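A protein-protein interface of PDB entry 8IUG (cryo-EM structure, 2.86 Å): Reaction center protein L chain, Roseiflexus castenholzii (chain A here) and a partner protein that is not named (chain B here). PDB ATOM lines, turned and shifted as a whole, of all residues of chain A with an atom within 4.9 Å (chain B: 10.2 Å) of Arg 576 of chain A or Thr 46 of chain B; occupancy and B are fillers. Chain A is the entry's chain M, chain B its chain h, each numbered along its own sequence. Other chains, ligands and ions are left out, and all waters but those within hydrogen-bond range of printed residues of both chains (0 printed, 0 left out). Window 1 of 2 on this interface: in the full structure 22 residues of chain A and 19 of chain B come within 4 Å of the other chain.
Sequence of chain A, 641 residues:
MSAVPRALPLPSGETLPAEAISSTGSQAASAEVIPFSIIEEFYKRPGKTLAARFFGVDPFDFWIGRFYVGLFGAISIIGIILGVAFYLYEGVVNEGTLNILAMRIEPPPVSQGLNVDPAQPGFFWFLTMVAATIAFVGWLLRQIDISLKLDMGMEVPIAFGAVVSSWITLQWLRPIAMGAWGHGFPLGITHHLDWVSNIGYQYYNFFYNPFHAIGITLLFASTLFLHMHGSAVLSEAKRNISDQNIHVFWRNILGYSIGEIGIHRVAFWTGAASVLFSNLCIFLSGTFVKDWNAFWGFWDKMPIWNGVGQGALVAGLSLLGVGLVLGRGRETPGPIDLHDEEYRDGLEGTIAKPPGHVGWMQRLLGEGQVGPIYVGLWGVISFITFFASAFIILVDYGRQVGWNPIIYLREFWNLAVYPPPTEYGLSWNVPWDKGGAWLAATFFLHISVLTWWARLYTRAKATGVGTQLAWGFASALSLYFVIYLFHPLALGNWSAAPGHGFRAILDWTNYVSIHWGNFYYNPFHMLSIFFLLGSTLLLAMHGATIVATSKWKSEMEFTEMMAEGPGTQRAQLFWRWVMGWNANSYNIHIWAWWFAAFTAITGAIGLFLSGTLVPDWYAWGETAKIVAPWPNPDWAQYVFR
Printed residues of chain B that touch a printed residue of chain A: Ala 38, Thr 41, Asp 42, Ala 45, Thr 46 and Tyr 49. Hydrophobic or aromatic side chains of chain B within 4 Å of the printed part of chain A: Ala 38, Ala 45 and Tyr 49. Hydrophobic or aromatic side chains of chain A within 4 Å of the printed part of chain B: Trp 581. Among the printed residues, no Asp or Glu carboxylate lies within 4 Å of a Lys or Arg side-chain nitrogen of the other chain.
Among the printed residues, pairs that only touch across the chains: Trp 581 of chain A with Asp 42 of chain B (3.3 Å), Asn 582 of chain A with Ala 45 of chain B (3.6 Å), Trp 581 of chain A with Ala 38 of chain B (3.7 Å), Gln 572 of chain A with Tyr 49 of chain B (3.7 Å), Gln 572 of chain A with Ala 45 of chain B (3.7 Å), Trp 581 of chain A with Thr 41 of chain B (3.8 Å), Arg 576 of chain A with Thr 46 of chain B (3.9 Å) and Asn 582 of chain A with Thr 46 of chain B (3.96 Å).
The side-chain carboxylate (OD1) of Asp 42 of chain B sits at hydrogen-bond distance from the backbone NH (N) of Asn 582 of chain A (3.2 Å).
The backbone carbonyl oxygen of Asp 42 of chain B sits at hydrogen-bond distance from the side-chain hydroxyl of Thr 46 of chain B, 2.8 Å away. O of Ala 45 of chain B sits at hydrogen-bond distance from OH of Tyr 49 of chain B. O of Ala 45 of chain B lies within hydrogen-bond range of NH2 of Arg 51 of chain B (3.5 Å). OH of Tyr 49 of chain B lies close to NH2 of Arg 51 of chain B (3.4 Å).
No residue of chain B comes within 4 Å of Gly 580 of chain A. Of the printed residues of chain B, Trp 581 of chain A touches Ala 38, Thr 41 and Asp 42. Printed residues of chain B within 4 Å of Asn 582 of chain A: Asp 42 (3.2 Å), Ala 45 (3.6 Å) and Thr 46 (3.96 Å). Of chain A, only Arg 576 (3.9 Å) and Asn 582 (3.96 Å) come within 4 Å of Thr 46 of chain B. The nearest printed residue of chain A that does not touch Thr 46 of chain B is Gln 572 of chain A (5.5 Å).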
ATOM      1  N   GLN A 572     -34.168  25.579  22.336  1.00  0.00           N
ATOM      2  CA  GLN A 572     -33.633  26.103  23.586  1.00  0.00           C
ATOM      3  C   GLN A 572     -34.720  26.230  24.640  1.00  0.00           C
ATOM      4  O   GLN A 572     -34.524  25.841  25.797  1.00  0.00           O
ATOM      5  CB  GLN A 572     -32.971  27.455  23.340  1.00  0.00           C
ATOM      6  CG  GLN A 572     -31.642  27.386  22.638  1.00  0.00           C
ATOM      7  CD  GLN A 572     -30.952  28.724  22.594  1.00  0.00           C
ATOM      8  OE1 GLN A 572     -31.586  29.753  22.385  1.00  0.00           O
ATOM      9  NE2 GLN A 572     -29.646  28.723  22.803  1.00  0.00           N
ATOM     10  N   LEU A 573     -35.878  26.777  24.260  1.00  0.00           N
ATOM     11  CA  LEU A 573     -36.963  26.945  25.222  1.00  0.00           C
ATOM     12  C   LEU A 573     -37.495  25.607  25.711  1.00  0.00           C
ATOM     13  O   LEU A 573     -37.810  25.459  26.895  1.00  0.00           O
ATOM     14  CB  LEU A 573     -38.086  27.779  24.612  1.00  0.00           C
ATOM     15  CG  LEU A 573     -37.773  29.264  24.463  1.00  0.00           C
ATOM     16  CD1 LEU A 573     -38.981  30.000  23.965  1.00  0.00           C
ATOM     17  CD2 LEU A 573     -37.315  29.840  25.782  1.00  0.00           C
ATOM     18  N   PHE A 574     -37.610  24.622  24.817  1.00  0.00           N
ATOM     19  CA  PHE A 574     -38.056  23.293  25.223  1.00  0.00           C
ATOM     20  C   PHE A 574     -37.152  22.722  26.303  1.00  0.00           C
ATOM     21  O   PHE A 574     -37.620  22.312  27.375  1.00  0.00           O
ATOM     22  CB  PHE A 574     -38.090  22.363  24.009  1.00  0.00           C
ATOM     23  CG  PHE A 574     -38.506  20.955  24.327  1.00  0.00           C
ATOM     24  CD1 PHE A 574     -39.840  20.597  24.325  1.00  0.00           C
ATOM     25  CD2 PHE A 574     -37.565  19.985  24.617  1.00  0.00           C
ATOM     26  CE1 PHE A 574     -40.222  19.308  24.617  1.00  0.00           C
ATOM     27  CE2 PHE A 574     -37.946  18.698  24.913  1.00  0.00           C
ATOM     28  CZ  PHE A 574     -39.274  18.360  24.911  1.00  0.00           C
ATOM     29  N   TRP A 575     -35.845  22.701  26.049  1.00  0.00           N
ATOM     30  CA  TRP A 575     -34.975  22.069  27.033  1.00  0.00           C
ATOM     31  C   TRP A 575     -34.794  22.920  28.284  1.00  0.00           C
ATOM     32  O   TRP A 575     -34.505  22.368  29.348  1.00  0.00           O
ATOM     33  CB  TRP A 575     -33.633  21.710  26.403  1.00  0.00           C
ATOM     34  CG  TRP A 575     -33.756  20.533  25.489  1.00  0.00           C
ATOM     35  CD1 TRP A 575     -33.682  20.540  24.133  1.00  0.00           C
ATOM     36  CD2 TRP A 575     -34.019  19.179  25.869  1.00  0.00           C
ATOM     37  NE1 TRP A 575     -33.862  19.274  23.642  1.00  0.00           N
ATOM     38  CE2 TRP A 575     -34.073  18.420  24.689  1.00  0.00           C
ATOM     39  CE3 TRP A 575     -34.211  18.534  27.094  1.00  0.00           C
ATOM     40  CZ2 TRP A 575     -34.305  17.052  24.697  1.00  0.00           C
ATOM     41  CZ3 TRP A 575     -34.444  17.181  27.097  1.00  0.00           C
ATOM     42  CH2 TRP A 575     -34.490  16.453  25.909  1.00  0.00           C
ATOM     43  N   ARG A 576     -34.997  24.238  28.200  1.00  0.00           N
ATOM     44  CA  ARG A 576     -34.956  25.058  29.406  1.00  0.00           C
ATOM     45  C   ARG A 576     -36.176  24.819  30.283  1.00  0.00           C
ATOM     46  O   ARG A 576     -36.055  24.732  31.508  1.00  0.00           O
ATOM     47  CB  ARG A 576     -34.846  26.533  29.035  1.00  0.00           C
ATOM     48  CG  ARG A 576     -35.140  27.480  30.176  1.00  0.00           C
ATOM     49  CD  ARG A 576     -34.452  28.805  29.973  1.00  0.00           C
ATOM     50  NE  ARG A 576     -34.973  29.837  30.857  1.00  0.00           N
ATOM     51  CZ  ARG A 576     -34.303  30.924  31.212  1.00  0.00           C
ATOM     52  NH1 ARG A 576     -33.061  31.131  30.812  1.00  0.00           N
ATOM     53  NH2 ARG A 576     -34.892  31.823  31.991  1.00  0.00           N
ATOM     54  N   TRP A 577     -37.361  24.710  29.680  1.00  0.00           N
ATOM     55  CA  TRP A 577     -38.567  24.455  30.459  1.00  0.00           C
ATOM     56  C   TRP A 577     -38.651  23.016  30.944  1.00  0.00           C
ATOM     57  O   TRP A 577     -39.425  22.737  31.861  1.00  0.00           O
ATOM     58  CB  TRP A 577     -39.809  24.805  29.640  1.00  0.00           C
ATOM     59  CG  TRP A 577     -39.916  26.260  29.306  1.00  0.00           C
ATOM     60  CD1 TRP A 577     -39.236  27.283  29.890  1.00  0.00           C
ATOM     61  CD2 TRP A 577     -40.748  26.854  28.303  1.00  0.00           C
ATOM     62  NE1 TRP A 577     -39.591  28.476  29.319  1.00  0.00           N
ATOM     63  CE2 TRP A 577     -40.518  28.240  28.341  1.00  0.00           C
ATOM     64  CE3 TRP A 577     -41.666  26.350  27.380  1.00  0.00           C
ATOM     65  CZ2 TRP A 577     -41.171  29.126  27.493  1.00  0.00           C
ATOM     66  CZ3 TRP A 577     -42.311  27.234  26.541  1.00  0.00           C
ATOM     67  CH2 TRP A 577     -42.060  28.604  26.602  1.00  0.00           C
ATOM     68  N   VAL A 578     -37.884  22.100  30.354  1.00  0.00           N
ATOM     69  CA  VAL A 578     -37.839  20.728  30.851  1.00  0.00           C
ATOM     70  C   VAL A 578     -36.788  20.570  31.948  1.00  0.00           C
ATOM     71  O   VAL A 578     -37.107  20.136  33.059  1.00  0.00           O
ATOM     72  CB  VAL A 578     -37.584  19.731  29.707  1.00  0.00           C
ATOM     73  CG1 VAL A 578     -37.266  18.362  30.263  1.00  0.00           C
ATOM     74  CG2 VAL A 578     -38.789  19.651  28.806  1.00  0.00           C
ATOM     75  N   MET A 579     -35.529  20.913  31.656  1.00  0.00           N
ATOM     76  CA  MET A 579     -34.430  20.636  32.576  1.00  0.00           C
ATOM     77  C   MET A 579     -34.008  21.821  33.431  1.00  0.00           C
ATOM     78  O   MET A 579     -33.339  21.615  34.446  1.00  0.00           O
ATOM     79  CB  MET A 579     -33.191  20.154  31.815  1.00  0.00           C
ATOM     80  CG  MET A 579     -33.122  18.680  31.569  1.00  0.00           C
ATOM     81  SD  MET A 579     -31.671  18.243  30.606  1.00  0.00           S
ATOM     82  CE  MET A 579     -31.356  19.782  29.765  1.00  0.00           C
ATOM     83  N   GLY A 580     -34.355  23.044  33.050  1.00  0.00           N
ATOM     84  CA  GLY A 580     -33.832  24.213  33.719  1.00  0.00           C
ATOM     85  C   GLY A 580     -32.547  24.761  33.138  1.00  0.00           C
ATOM     86  O   GLY A 580     -32.058  25.784  33.627  1.00  0.00           O
ATOM     87  N   TRP A 581     -31.979  24.115  32.123  1.00  0.00           N
ATOM     88  CA  TRP A 581     -30.807  24.635  31.438  1.00  0.00           C
ATOM     89  C   TRP A 581     -30.781  24.075  30.024  1.00  0.00           C
ATOM     90  O   TRP A 581     -31.378  23.037  29.739  1.00  0.00           O
ATOM     91  CB  TRP A 581     -29.513  24.307  32.202  1.00  0.00           C
ATOM     92  CG  TRP A 581     -29.231  22.846  32.409  1.00  0.00           C
ATOM     93  CD1 TRP A 581     -29.912  21.984  33.212  1.00  0.00           C
ATOM     94  CD2 TRP A 581     -28.166  22.091  31.826  1.00  0.00           C
ATOM     95  NE1 TRP A 581     -29.354  20.736  33.151  1.00  0.00           N
ATOM     96  CE2 TRP A 581     -28.278  20.775  32.306  1.00  0.00           C
ATOM     97  CE3 TRP A 581     -27.135  22.398  30.934  1.00  0.00           C
ATOM     98  CZ2 TRP A 581     -27.399  19.769  31.926  1.00  0.00           C
ATOM     99  CZ3 TRP A 581     -26.268  21.401  30.561  1.00  0.00           C
ATOM    100  CH2 TRP A 581     -26.402  20.102  31.057  1.00  0.00           C
ATOM    101  N   ASN A 582     -30.087  24.784  29.132  1.00  0.00           N
ATOM    102  CA  ASN A 582     -30.037  24.423  27.718  1.00  0.00           C
ATOM    103  C   ASN A 582     -28.648  24.754  27.176  1.00  0.00           C
ATOM    104  O   ASN A 582     -27.721  25.062  27.928  1.00  0.00           O
ATOM    105  CB  ASN A 582     -31.155  25.127  26.936  1.00  0.00           C
ATOM    106  CG  ASN A 582     -31.027  26.637  26.950  1.00  0.00           C
ATOM    107  OD1 ASN A 582     -31.553  27.306  27.832  1.00  0.00           O
ATOM    108  ND2 ASN A 582     -30.336  27.181  25.965  1.00  0.00           N
ATOM    109  N   ALA B  38     -21.796  22.147  32.704  1.00  0.00           N
ATOM    110  CA  ALA B  38     -23.184  22.570  32.560  1.00  0.00           C
ATOM    111  C   ALA B  38     -23.345  24.050  32.873  1.00  0.00           C
ATOM    112  O   ALA B  38     -24.043  24.774  32.151  1.00  0.00           O
ATOM    113  CB  ALA B  38     -24.077  21.727  33.465  1.00  0.00           C
ATOM    114  N   ARG B  39     -22.697  24.520  33.941  1.00  0.00           N
ATOM    115  CA  ARG B  39     -22.753  25.936  34.286  1.00  0.00           C
ATOM    116  C   ARG B  39     -22.264  26.803  33.132  1.00  0.00           C
ATOM    117  O   ARG B  39     -22.926  27.773  32.745  1.00  0.00           O
ATOM    118  CB  ARG B  39     -21.929  26.188  35.550  1.00  0.00           C
ATOM    119  CG  ARG B  39     -21.494  27.628  35.773  1.00  0.00           C
ATOM    120  CD  ARG B  39     -22.676  28.551  35.965  1.00  0.00           C
ATOM    121  NE  ARG B  39     -22.267  29.935  36.161  1.00  0.00           N
ATOM    122  CZ  ARG B  39     -23.024  30.983  35.873  1.00  0.00           C
ATOM    123  NH1 ARG B  39     -24.221  30.841  35.330  1.00  0.00           N
ATOM    124  NH2 ARG B  39     -22.566  32.204  36.126  1.00  0.00           N
ATOM    125  N   PHE B  40     -21.124  26.447  32.540  1.00  0.00           N
ATOM    126  CA  PHE B  40     -20.549  27.311  31.510  1.00  0.00           C
ATOM    127  C   PHE B  40     -21.312  27.223  30.190  1.00  0.00           C
ATOM    128  O   PHE B  40     -21.457  28.232  29.485  1.00  0.00           O
ATOM    129  CB  PHE B  40     -19.071  26.991  31.320  1.00  0.00           C
ATOM    130  CG  PHE B  40     -18.194  27.642  32.344  1.00  0.00           C
ATOM    131  CD1 PHE B  40     -17.886  28.986  32.248  1.00  0.00           C
ATOM    132  CD2 PHE B  40     -17.701  26.925  33.416  1.00  0.00           C
ATOM    133  CE1 PHE B  40     -17.094  29.596  33.191  1.00  0.00           C
ATOM    134  CE2 PHE B  40     -16.906  27.534  34.363  1.00  0.00           C
ATOM    135  CZ  PHE B  40     -16.604  28.868  34.250  1.00  0.00           C
ATOM    136  N   THR B  41     -21.828  26.044  29.837  1.00  0.00           N
ATOM    137  CA  THR B  41     -22.596  25.949  28.600  1.00  0.00           C
ATOM    138  C   THR B  41     -23.924  26.691  28.718  1.00  0.00           C
ATOM    139  O   THR B  41     -24.362  27.341  27.760  1.00  0.00           O
ATOM    140  CB  THR B  41     -22.801  24.484  28.197  1.00  0.00           C
ATOM    141  OG1 THR B  41     -23.426  24.427  26.914  1.00  0.00           O
ATOM    142  CG2 THR B  41     -23.674  23.753  29.164  1.00  0.00           C
ATOM    143  N   ASP B  42     -24.565  26.641  29.891  1.00  0.00           N
ATOM    144  CA  ASP B  42     -25.790  27.410  30.073  1.00  0.00           C
ATOM    145  C   ASP B  42     -25.506  28.904  30.141  1.00  0.00           C
ATOM    146  O   ASP B  42     -26.347  29.709  29.733  1.00  0.00           O
ATOM    147  CB  ASP B  42     -26.520  26.947  31.331  1.00  0.00           C
ATOM    148  CG  ASP B  42     -27.859  27.628  31.511  1.00  0.00           C
ATOM    149  OD1 ASP B  42     -28.820  27.244  30.815  1.00  0.00           O
ATOM    150  OD2 ASP B  42     -27.956  28.544  32.348  1.00  0.00           O
ATOM    151  N   LYS B  43     -24.342  29.295  30.665  1.00  0.00           N
ATOM    152  CA  LYS B  43     -23.974  30.706  30.663  1.00  0.00           C
ATOM    153  C   LYS B  43     -23.789  31.230  29.246  1.00  0.00           C
ATOM    154  O   LYS B  43     -24.232  32.338  28.924  1.00  0.00           O
ATOM    155  CB  LYS B  43     -22.700  30.910  31.477  1.00  0.00           C
ATOM    156  CG  LYS B  43     -22.308  32.357  31.654  1.00  0.00           C
ATOM    157  CD  LYS B  43     -20.909  32.475  32.210  1.00  0.00           C
ATOM    158  CE  LYS B  43     -20.593  33.909  32.577  1.00  0.00           C
ATOM    159  NZ  LYS B  43     -20.732  34.814  31.406  1.00  0.00           N
ATOM    160  N   GLN B  44     -23.125  30.455  28.387  1.00  0.00           N
ATOM    161  CA  GLN B  44     -22.935  30.892  27.005  1.00  0.00           C
ATOM    162  C   GLN B  44     -24.248  30.894  26.230  1.00  0.00           C
ATOM    163  O   GLN B  44     -24.497  31.800  25.429  1.00  0.00           O
ATOM    164  CB  GLN B  44     -21.903  30.004  26.313  1.00  0.00           C
ATOM    165  CG  GLN B  44     -21.836  30.160  24.802  1.00  0.00           C
ATOM    166  CD  GLN B  44     -21.376  31.536  24.359  1.00  0.00           C
ATOM    167  OE1 GLN B  44     -20.631  32.213  25.063  1.00  0.00           O
ATOM    168  NE2 GLN B  44     -21.821  31.954  23.182  1.00  0.00           N
ATOM    169  N   ALA B  45     -25.104  29.896  26.462  1.00  0.00           N
ATOM    170  CA  ALA B  45     -26.312  29.748  25.655  1.00  0.00           C
ATOM    171  C   ALA B  45     -27.283  30.908  25.842  1.00  0.00           C
ATOM    172  O   ALA B  45     -27.955  31.320  24.891  1.00  0.00           O
ATOM    173  CB  ALA B  45     -27.000  28.431  25.993  1.00  0.00           C
ATOM    174  N   THR B  46     -27.395  31.434  27.062  1.00  0.00           N
ATOM    175  CA  THR B  46     -28.422  32.411  27.401  1.00  0.00           C
ATOM    176  C   THR B  46     -27.897  33.841  27.424  1.00  0.00           C
ATOM    177  O   THR B  46     -28.372  34.658  28.216  1.00  0.00           O
ATOM    178  CB  THR B  46     -29.056  32.066  28.747  1.00  0.00           C
ATOM    179  OG1 THR B  46     -28.031  31.888  29.729  1.00  0.00           O
ATOM    180  CG2 THR B  46     -29.867  30.793  28.646  1.00  0.00           C
ATOM    181  N   SER B  47     -26.933  34.164  26.571  1.00  0.00           N
ATOM    182  CA  SER B  47     -26.396  35.511  26.488  1.00  0.00           C
ATOM    183  C   SER B  47     -26.988  36.233  25.281  1.00  0.00           C
ATOM    184  O   SER B  47     -27.869  35.724  24.586  1.00  0.00           O
ATOM    185  CB  SER B  47     -24.870  35.479  26.423  1.00  0.00           C
ATOM    186  OG  SER B  47     -24.423  34.724  25.318  1.00  0.00           O
ATOM    187  N   ALA B  48     -26.494  37.442  25.033  1.00  0.00           N
ATOM    188  CA  ALA B  48     -27.012  38.299  23.976  1.00  0.00           C
ATOM    189  C   ALA B  48     -26.096  38.221  22.763  1.00  0.00           C
ATOM    190  O   ALA B  48     -24.929  38.614  22.836  1.00  0.00           O
ATOM    191  CB  ALA B  48     -27.134  39.742  24.459  1.00  0.00           C
ATOM    192  N   TYR B  49     -26.628  37.714  21.655  1.00  0.00           N
ATOM    193  CA  TYR B  49     -25.901  37.654  20.397  1.00  0.00           C
ATOM    194  C   TYR B  49     -26.912  37.745  19.262  1.00  0.00           C
ATOM    195  O   TYR B  49     -28.108  37.941  19.490  1.00  0.00           O
ATOM    196  CB  TYR B  49     -25.031  36.392  20.317  1.00  0.00           C
ATOM    197  CG  TYR B  49     -25.697  35.096  20.722  1.00  0.00           C
ATOM    198  CD1 TYR B  49     -26.660  34.508  19.924  1.00  0.00           C
ATOM    199  CD2 TYR B  49     -25.330  34.446  21.886  1.00  0.00           C
ATOM    200  CE1 TYR B  49     -27.252  33.325  20.285  1.00  0.00           C
ATOM    201  CE2 TYR B  49     -25.916  33.266  22.253  1.00  0.00           C
ATOM    202  CZ  TYR B  49     -26.876  32.709  21.451  1.00  0.00           C
ATOM    203  OH  TYR B  49     -27.467  31.524  21.812  1.00  0.00           O
ATOM    204  N   ARG B  51     -29.610  37.208  16.769  1.00  0.00           N
ATOM    205  CA  ARG B  51     -30.776  36.354  16.620  1.00  0.00           C
ATOM    206  C   ARG B  51     -31.725  37.009  15.630  1.00  0.00           C
ATOM    207  O   ARG B  51     -31.700  38.225  15.435  1.00  0.00           O
ATOM    208  CB  ARG B  51     -31.492  36.122  17.959  1.00  0.00           C
ATOM    209  CG  ARG B  51     -30.694  35.354  18.998  1.00  0.00           C
ATOM    210  CD  ARG B  51     -31.436  35.323  20.323  1.00  0.00           C
ATOM    211  NE  ARG B  51     -30.849  34.395  21.283  1.00  0.00           N
ATOM    212  CZ  ARG B  51     -30.088  34.749  22.309  1.00  0.00           C
ATOM    213  NH1 ARG B  51     -29.780  36.013  22.536  1.00  0.00           N
ATOM    214  NH2 ARG B  51     -29.630  33.813  23.130  1.00  0.00           N
